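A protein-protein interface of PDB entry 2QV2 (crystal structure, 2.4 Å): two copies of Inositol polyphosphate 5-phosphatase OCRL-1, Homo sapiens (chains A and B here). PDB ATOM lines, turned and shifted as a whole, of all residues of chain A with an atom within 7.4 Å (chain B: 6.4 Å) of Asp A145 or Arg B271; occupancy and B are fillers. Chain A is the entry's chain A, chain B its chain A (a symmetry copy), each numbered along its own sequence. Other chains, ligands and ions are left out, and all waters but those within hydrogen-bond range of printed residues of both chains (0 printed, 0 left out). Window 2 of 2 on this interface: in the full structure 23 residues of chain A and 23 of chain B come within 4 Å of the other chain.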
ATOM      1  N   VAL A 140     -25.617  11.649 -22.313  1.00  0.00           N
ATOM      2  CA  VAL A 140     -25.225  13.029 -22.610  1.00  0.00           C
ATOM      3  C   VAL A 140     -26.398  14.005 -22.454  1.00  0.00           C
ATOM      4  O   VAL A 140     -26.402  15.104 -23.012  1.00  0.00           O
ATOM      5  CB  VAL A 140     -24.637  13.158 -24.038  1.00  0.00           C
ATOM      6  CG1 VAL A 140     -23.374  12.338 -24.149  1.00  0.00           C
ATOM      7  CG2 VAL A 140     -25.653  12.714 -25.073  1.00  0.00           C
ATOM      8  N   THR A 141     -27.376  13.586 -21.660  1.00  0.00           N
ATOM      9  CA  THR A 141     -28.588  14.351 -21.400  1.00  0.00           C
ATOM     10  C   THR A 141     -28.397  15.805 -20.970  1.00  0.00           C
ATOM     11  O   THR A 141     -29.074  16.696 -21.483  1.00  0.00           O
ATOM     12  CB  THR A 141     -29.444  13.633 -20.336  1.00  0.00           C
ATOM     13  OG1 THR A 141     -29.848  12.354 -20.840  1.00  0.00           O
ATOM     14  CG2 THR A 141     -30.676  14.450 -19.997  1.00  0.00           C
ATOM     15  N   LYS A 142     -27.490  16.046 -20.031  1.00  0.00           N
ATOM     16  CA  LYS A 142     -27.249  17.397 -19.539  1.00  0.00           C
ATOM     17  C   LYS A 142     -26.534  18.317 -20.536  1.00  0.00           C
ATOM     18  O   LYS A 142     -26.247  19.473 -20.223  1.00  0.00           O
ATOM     19  CB  LYS A 142     -26.465  17.336 -18.225  1.00  0.00           C
ATOM     20  CG  LYS A 142     -27.174  16.532 -17.142  1.00  0.00           C
ATOM     21  CD  LYS A 142     -26.435  16.576 -15.812  1.00  0.00           C
ATOM     22  CE  LYS A 142     -26.524  17.950 -15.169  1.00  0.00           C
ATOM     23  NZ  LYS A 142     -27.929  18.327 -14.855  1.00  0.00           N
ATOM     24  N   LEU A 143     -26.250  17.804 -21.729  1.00  0.00           N
ATOM     25  CA  LEU A 143     -25.586  18.589 -22.761  1.00  0.00           C
ATOM     26  C   LEU A 143     -26.562  18.948 -23.874  1.00  0.00           C
ATOM     27  O   LEU A 143     -26.394  19.959 -24.549  1.00  0.00           O
ATOM     28  CB  LEU A 143     -24.390  17.823 -23.351  1.00  0.00           C
ATOM     29  CG  LEU A 143     -23.129  17.677 -22.490  1.00  0.00           C
ATOM     30  CD1 LEU A 143     -23.460  16.907 -21.232  1.00  0.00           C
ATOM     31  CD2 LEU A 143     -22.062  16.940 -23.247  1.00  0.00           C
ATOM     32  N   ILE A 144     -27.585  18.118 -24.061  1.00  0.00           N
ATOM     33  CA  ILE A 144     -28.586  18.357 -25.102  1.00  0.00           C
ATOM     34  C   ILE A 144     -29.150  19.775 -25.047  1.00  0.00           C
ATOM     35  O   ILE A 144     -29.596  20.249 -23.996  1.00  0.00           O
ATOM     36  CB  ILE A 144     -29.751  17.357 -25.003  1.00  0.00           C
ATOM     37  CG1 ILE A 144     -29.239  15.935 -25.232  1.00  0.00           C
ATOM     38  CG2 ILE A 144     -30.800  17.688 -26.045  1.00  0.00           C
ATOM     39  CD1 ILE A 144     -30.314  14.881 -25.160  1.00  0.00           C
ATOM     40  N   ASP A 145     -29.131  20.436 -26.199  1.00  0.00           N
ATOM     41  CA  ASP A 145     -29.601  21.811 -26.330  1.00  0.00           C
ATOM     42  C   ASP A 145     -31.027  21.914 -26.874  1.00  0.00           C
ATOM     43  O   ASP A 145     -31.224  22.130 -28.070  1.00  0.00           O
ATOM     44  CB  ASP A 145     -28.640  22.577 -27.244  1.00  0.00           C
ATOM     45  CG  ASP A 145     -29.024  24.028 -27.414  1.00  0.00           C
ATOM     46  OD1 ASP A 145     -29.056  24.754 -26.399  1.00  0.00           O
ATOM     47  OD2 ASP A 145     -29.287  24.442 -28.564  1.00  0.00           O
ATOM     48  N   LEU A 146     -32.020  21.770 -25.997  1.00  0.00           N
ATOM     49  CA  LEU A 146     -33.417  21.860 -26.413  1.00  0.00           C
ATOM     50  C   LEU A 146     -34.358  21.998 -25.219  1.00  0.00           C
ATOM     51  O   LEU A 146     -33.937  21.885 -24.067  1.00  0.00           O
ATOM     52  CB  LEU A 146     -33.804  20.622 -27.237  1.00  0.00           C
ATOM     53  CG  LEU A 146     -34.322  19.331 -26.575  1.00  0.00           C
ATOM     54  CD1 LEU A 146     -33.584  19.064 -25.273  1.00  0.00           C
ATOM     55  CD2 LEU A 146     -35.815  19.450 -26.319  1.00  0.00           C
ATOM     56  N   GLU A 147     -35.633  22.242 -25.506  1.00  0.00           N
ATOM     57  CA  GLU A 147     -36.648  22.379 -24.468  1.00  0.00           C
ATOM     58  C   GLU A 147     -37.859  21.505 -24.768  1.00  0.00           C
ATOM     59  O   GLU A 147     -38.655  21.813 -25.654  1.00  0.00           O
ATOM     60  CB  GLU A 147     -37.086  23.840 -24.333  1.00  0.00           C
ATOM     61  CG  GLU A 147     -36.143  24.693 -23.501  1.00  0.00           C
ATOM     62  CD  GLU A 147     -36.068  24.238 -22.049  1.00  0.00           C
ATOM     63  OE1 GLU A 147     -35.326  24.865 -21.264  1.00  0.00           O
ATOM     64  OE2 GLU A 147     -36.750  23.254 -21.691  1.00  0.00           O
ATOM     65  N   GLU B 126     -18.024  22.621 -34.084  1.00  0.00           N
ATOM     66  CA  GLU B 126     -19.267  22.585 -34.846  1.00  0.00           C
ATOM     67  C   GLU B 126     -19.656  21.144 -35.151  1.00  0.00           C
ATOM     68  O   GLU B 126     -20.760  20.702 -34.845  1.00  0.00           O
ATOM     69  CB  GLU B 126     -19.078  23.352 -36.156  1.00  0.00           C
ATOM     70  CG  GLU B 126     -20.339  23.981 -36.723  1.00  0.00           C
ATOM     71  CD  GLU B 126     -20.824  25.158 -35.895  1.00  0.00           C
ATOM     72  OE1 GLU B 126     -21.314  24.935 -34.766  1.00  0.00           O
ATOM     73  OE2 GLU B 126     -20.709  26.309 -36.372  1.00  0.00           O
ATOM     74  N   ARG B 171     -30.918  17.988 -32.405  1.00  0.00           N
ATOM     75  CA  ARG B 171     -30.496  19.178 -31.670  1.00  0.00           C
ATOM     76  C   ARG B 171     -29.032  19.007 -31.255  1.00  0.00           C
ATOM     77  O   ARG B 171     -28.686  18.084 -30.510  1.00  0.00           O
ATOM     78  CB  ARG B 171     -31.353  19.382 -30.414  1.00  0.00           C
ATOM     79  CG  ARG B 171     -32.846  19.485 -30.670  1.00  0.00           C
ATOM     80  CD  ARG B 171     -33.543  18.145 -30.476  1.00  0.00           C
ATOM     81  NE  ARG B 171     -33.542  17.728 -29.075  1.00  0.00           N
ATOM     82  CZ  ARG B 171     -34.138  16.631 -28.617  1.00  0.00           C
ATOM     83  NH1 ARG B 171     -34.788  15.829 -29.449  1.00  0.00           N
ATOM     84  NH2 ARG B 171     -34.086  16.337 -27.324  1.00  0.00           N
ATOM     85  N   PRO B 172     -28.150  19.897 -31.731  1.00  0.00           N
ATOM     86  CA  PRO B 172     -26.732  19.801 -31.381  1.00  0.00           C
ATOM     87  C   PRO B 172     -26.530  19.984 -29.883  1.00  0.00           C
ATOM     88  O   PRO B 172     -27.303  20.688 -29.230  1.00  0.00           O
ATOM     89  CB  PRO B 172     -26.110  20.926 -32.200  1.00  0.00           C
ATOM     90  CG  PRO B 172     -27.185  21.958 -32.190  1.00  0.00           C
ATOM     91  CD  PRO B 172     -28.419  21.137 -32.477  1.00  0.00           C
ATOM     92  N   LEU B 173     -25.503  19.338 -29.337  1.00  0.00           N
ATOM     93  CA  LEU B 173     -25.212  19.451 -27.909  1.00  0.00           C
ATOM     94  C   LEU B 173     -24.717  20.871 -27.619  1.00  0.00           C
ATOM     95  O   LEU B 173     -24.186  21.537 -28.504  1.00  0.00           O
ATOM     96  CB  LEU B 173     -24.130  18.442 -27.510  1.00  0.00           C
ATOM     97  CG  LEU B 173     -24.292  17.003 -28.006  1.00  0.00           C
ATOM     98  CD1 LEU B 173     -23.034  16.229 -27.692  1.00  0.00           C
ATOM     99  CD2 LEU B 173     -25.504  16.348 -27.360  1.00  0.00           C
ATOM    100  N   GLN B 174     -24.898  21.337 -26.392  1.00  0.00           N
ATOM    101  CA  GLN B 174     -24.456  22.676 -26.024  1.00  0.00           C
ATOM    102  C   GLN B 174     -22.940  22.771 -26.092  1.00  0.00           C
ATOM    103  O   GLN B 174     -22.386  23.832 -26.355  1.00  0.00           O
ATOM    104  CB  GLN B 174     -24.904  23.012 -24.607  1.00  0.00           C
ATOM    105  CG  GLN B 174     -26.388  22.904 -24.388  1.00  0.00           C
ATOM    106  CD  GLN B 174     -26.757  23.147 -22.948  1.00  0.00           C
ATOM    107  OE1 GLN B 174     -27.631  22.479 -22.393  1.00  0.00           O
ATOM    108  NE2 GLN B 174     -26.090  24.109 -22.327  1.00  0.00           N
ATOM    109  N   LEU B 269     -20.267  35.230 -30.819  1.00  0.00           N
ATOM    110  CA  LEU B 269     -19.758  33.939 -31.278  1.00  0.00           C
ATOM    111  C   LEU B 269     -20.846  32.949 -31.647  1.00  0.00           C
ATOM    112  O   LEU B 269     -21.951  32.998 -31.121  1.00  0.00           O
ATOM    113  CB  LEU B 269     -18.897  33.294 -30.184  1.00  0.00           C
ATOM    114  CG  LEU B 269     -17.536  33.885 -29.804  1.00  0.00           C
ATOM    115  CD1 LEU B 269     -17.060  33.251 -28.513  1.00  0.00           C
ATOM    116  CD2 LEU B 269     -16.539  33.645 -30.918  1.00  0.00           C
ATOM    117  N   PRO B 270     -20.546  32.028 -32.563  1.00  0.00           N
ATOM    118  CA  PRO B 270     -21.591  31.056 -32.906  1.00  0.00           C
ATOM    119  C   PRO B 270     -21.953  30.314 -31.610  1.00  0.00           C
ATOM    120  O   PRO B 270     -21.153  30.272 -30.667  1.00  0.00           O
ATOM    121  CB  PRO B 270     -20.905  30.139 -33.917  1.00  0.00           C
ATOM    122  CG  PRO B 270     -19.872  31.047 -34.578  1.00  0.00           C
ATOM    123  CD  PRO B 270     -19.361  31.907 -33.438  1.00  0.00           C
ATOM    124  N   ARG B 271     -23.149  29.731 -31.572  1.00  0.00           N
ATOM    125  CA  ARG B 271     -23.660  29.006 -30.402  1.00  0.00           C
ATOM    126  C   ARG B 271     -22.669  28.141 -29.598  1.00  0.00           C
ATOM    127  O   ARG B 271     -22.359  28.439 -28.441  1.00  0.00           O
ATOM    128  CB  ARG B 271     -24.852  28.145 -30.830  1.00  0.00           C
ATOM    129  CG  ARG B 271     -26.122  28.372 -30.022  1.00  0.00           C
ATOM    130  CD  ARG B 271     -26.080  27.679 -28.669  1.00  0.00           C
ATOM    131  NE  ARG B 271     -27.154  28.133 -27.785  1.00  0.00           N
ATOM    132  CZ  ARG B 271     -27.379  27.654 -26.564  1.00  0.00           C
ATOM    133  NH1 ARG B 271     -26.610  26.693 -26.066  1.00  0.00           N
ATOM    134  NH2 ARG B 271     -28.362  28.151 -25.826  1.00  0.00           N
ATOM    135  N   CYS B 272     -22.168  27.074 -30.204  1.00  0.00           N
ATOM    136  CA  CYS B 272     -21.263  26.189 -29.489  1.00  0.00           C
ATOM    137  C   CYS B 272     -19.935  26.818 -29.052  1.00  0.00           C
ATOM    138  O   CYS B 272     -19.351  26.402 -28.044  1.00  0.00           O
ATOM    139  CB  CYS B 272     -21.012  24.931 -30.313  1.00  0.00           C
ATOM    140  SG  CYS B 272     -20.279  25.257 -31.889  1.00  0.00           S
ATOM    141  N   HIS B 273     -19.457  27.817 -29.790  1.00  0.00           N
ATOM    142  CA  HIS B 273     -18.205  28.470 -29.421  1.00  0.00           C
ATOM    143  C   HIS B 273     -18.403  29.301 -28.167  1.00  0.00           C
ATOM    144  O   HIS B 273     -17.529  29.350 -27.314  1.00  0.00           O
ATOM    145  CB  HIS B 273     -17.691  29.354 -30.559  1.00  0.00           C
ATOM    146  CG  HIS B 273     -16.974  28.595 -31.634  1.00  0.00           C
ATOM    147  ND1 HIS B 273     -15.613  28.688 -31.829  1.00  0.00           N
ATOM    148  CD2 HIS B 273     -17.424  27.708 -32.553  1.00  0.00           C
ATOM    149  CE1 HIS B 273     -15.255  27.889 -32.820  1.00  0.00           C
ATOM    150  NE2 HIS B 273     -16.336  27.282 -33.277  1.00  0.00           N
ATOM    151  N   ARG B 274     -19.563  29.936 -28.041  1.00  0.00           N
ATOM    152  CA  ARG B 274     -19.831  30.759 -26.869  1.00  0.00           C
ATOM    153  C   ARG B 274     -20.060  29.890 -25.640  1.00  0.00           C
ATOM    154  O   ARG B 274     -19.656  30.249 -24.530  1.00  0.00           O
ATOM    155  CB  ARG B 274     -21.045  31.672 -27.101  1.00  0.00           C
ATOM    156  CG  ARG B 274     -22.397  30.992 -27.019  1.00  0.00           C
ATOM    157  CD  ARG B 274     -23.533  32.024 -27.005  1.00  0.00           C
ATOM    158  NE  ARG B 274     -23.706  32.678 -28.301  1.00  0.00           N
ATOM    159  CZ  ARG B 274     -24.752  32.492 -29.100  1.00  0.00           C
ATOM    160  NH1 ARG B 274     -25.734  31.676 -28.740  1.00  0.00           N
ATOM    161  NH2 ARG B 274     -24.809  33.117 -30.270  1.00  0.00           N
ATOM    162  N   ASN B 275     -20.708  28.746 -25.833  1.00  0.00           N
ATOM    163  CA  ASN B 275     -20.952  27.841 -24.720  1.00  0.00           C
ATOM    164  C   ASN B 275     -19.630  27.242 -24.250  1.00  0.00           C
ATOM    165  O   ASN B 275     -19.383  27.132 -23.050  1.00  0.00           O
ATOM    166  CB  ASN B 275     -21.879  26.688 -25.114  1.00  0.00           C
ATOM    167  CG  ASN B 275     -23.267  27.144 -25.500  1.00  0.00           C
ATOM    168  OD1 ASN B 275     -23.772  28.156 -25.008  1.00  0.00           O
ATOM    169  ND2 ASN B 275     -23.908  26.373 -26.374  1.00  0.00           N
ATOM    170  N   VAL B 276     -18.785  26.840 -25.194  1.00  0.00           N
ATOM    171  CA  VAL B 276     -17.524  26.247 -24.814  1.00  0.00           C
ATOM    172  C   VAL B 276     -16.690  27.289 -24.099  1.00  0.00           C
ATOM    173  O   VAL B 276     -16.042  26.988 -23.088  1.00  0.00           O
ATOM    174  CB  VAL B 276     -16.748  25.694 -26.024  1.00  0.00           C
ATOM    175  CG1 VAL B 276     -15.334  25.343 -25.605  1.00  0.00           C
ATOM    176  CG2 VAL B 276     -17.436  24.439 -26.562  1.00  0.00           C
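The backbone carbonyl oxygen (O) of Leu A143 lies within hydrogen-bond range of the backbone NH (N) of Gln B174 (2.7 Å).
The backbone carbonyl oxygen (O) of Ile A144 lies close to the side-chain amide oxygen (OE1) of Gln B174 (3.4 Å).
The side-chain carboxylate of Asp A145 lies within salt-bridge range of the guanidinium group of Arg B271 (3.1 Å).
The backbone carbonyl oxygen (O) of Gln B174 lies within hydrogen-bond range of the side-chain amide nitrogen (ND2) of Asn B275, at 3.0 Å.
NH1 of Arg B271 sits close to ND2 of Asn B275, at 2.7 Å.
Printed residues of chain B that touch a printed residue of chain A: Arg B171, Pro B172, Leu B173, Gln B174 and Arg B271.
Along chain B the printed residues that touch a printed residue of chain A span positions 171 to 271.
Printed residues of chain A that touch a printed residue of chain B: Lys A142, Leu A143, Ile A144, Asp A145 and Leu A146.
Along chain A the printed residues that touch a printed residue of chain B span positions 142 to 146.
Among the printed residues, Asp or Glu carboxylates within 4 Å of a Lys or Arg side-chain nitrogen of the other chain: Asp A145 with Arg B271.
No position is printed for both chains.
Of the 10 pairs that touch across the chains among the printed residues, none has its exchanged pair printed and touching as well.
Printed residues of chain B within 4 Å of Leu A143: Leu B173 and Gln B174.
Of chain B, only Arg B171 (3.6 Å), Pro B172 (3.0 Å), Gln B174 (3.7 Å) and Arg B271 (3.1 Å) come within 4 Å of Asp A145.
Of the printed residues of chain B, Leu A146 touches Arg B171.
Glu B126 touches none of the printed residues of chain A.
Printed residues of chain A within 4 Å of Arg B171: Ile A144 (3.8 Å), Asp A145 (3.6 Å) and Leu A146 (3.1 Å).
Printed residues of chain A within 4 Å of Pro B172: Asp A145.
Printed residues of chain A within 4 Å of Gln B174: Lys A142 (3.96 Å), Leu A143 (2.7 Å), Ile A144 (3.4 Å) and Asp A145 (3.7 Å).
Of chain A, only Asp A145 (3.1 Å) comes within 4 Å of Arg B271.
Val B276 touches none of the printed residues of chain A.
Lys A142 touches Gln B174 (O to OE1, 3.96 Å).
Leu A143 touches Leu B173.
CG2 of Ile A144 touches NH2 of Arg B171, 3.8 Å away.
Asp A145 touches Arg B171 (O to CB, 3.6 Å).
Pro B172 touches Asp A145.
Gln B174 touches Asp A145.
Arg B171 touches Leu A146.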
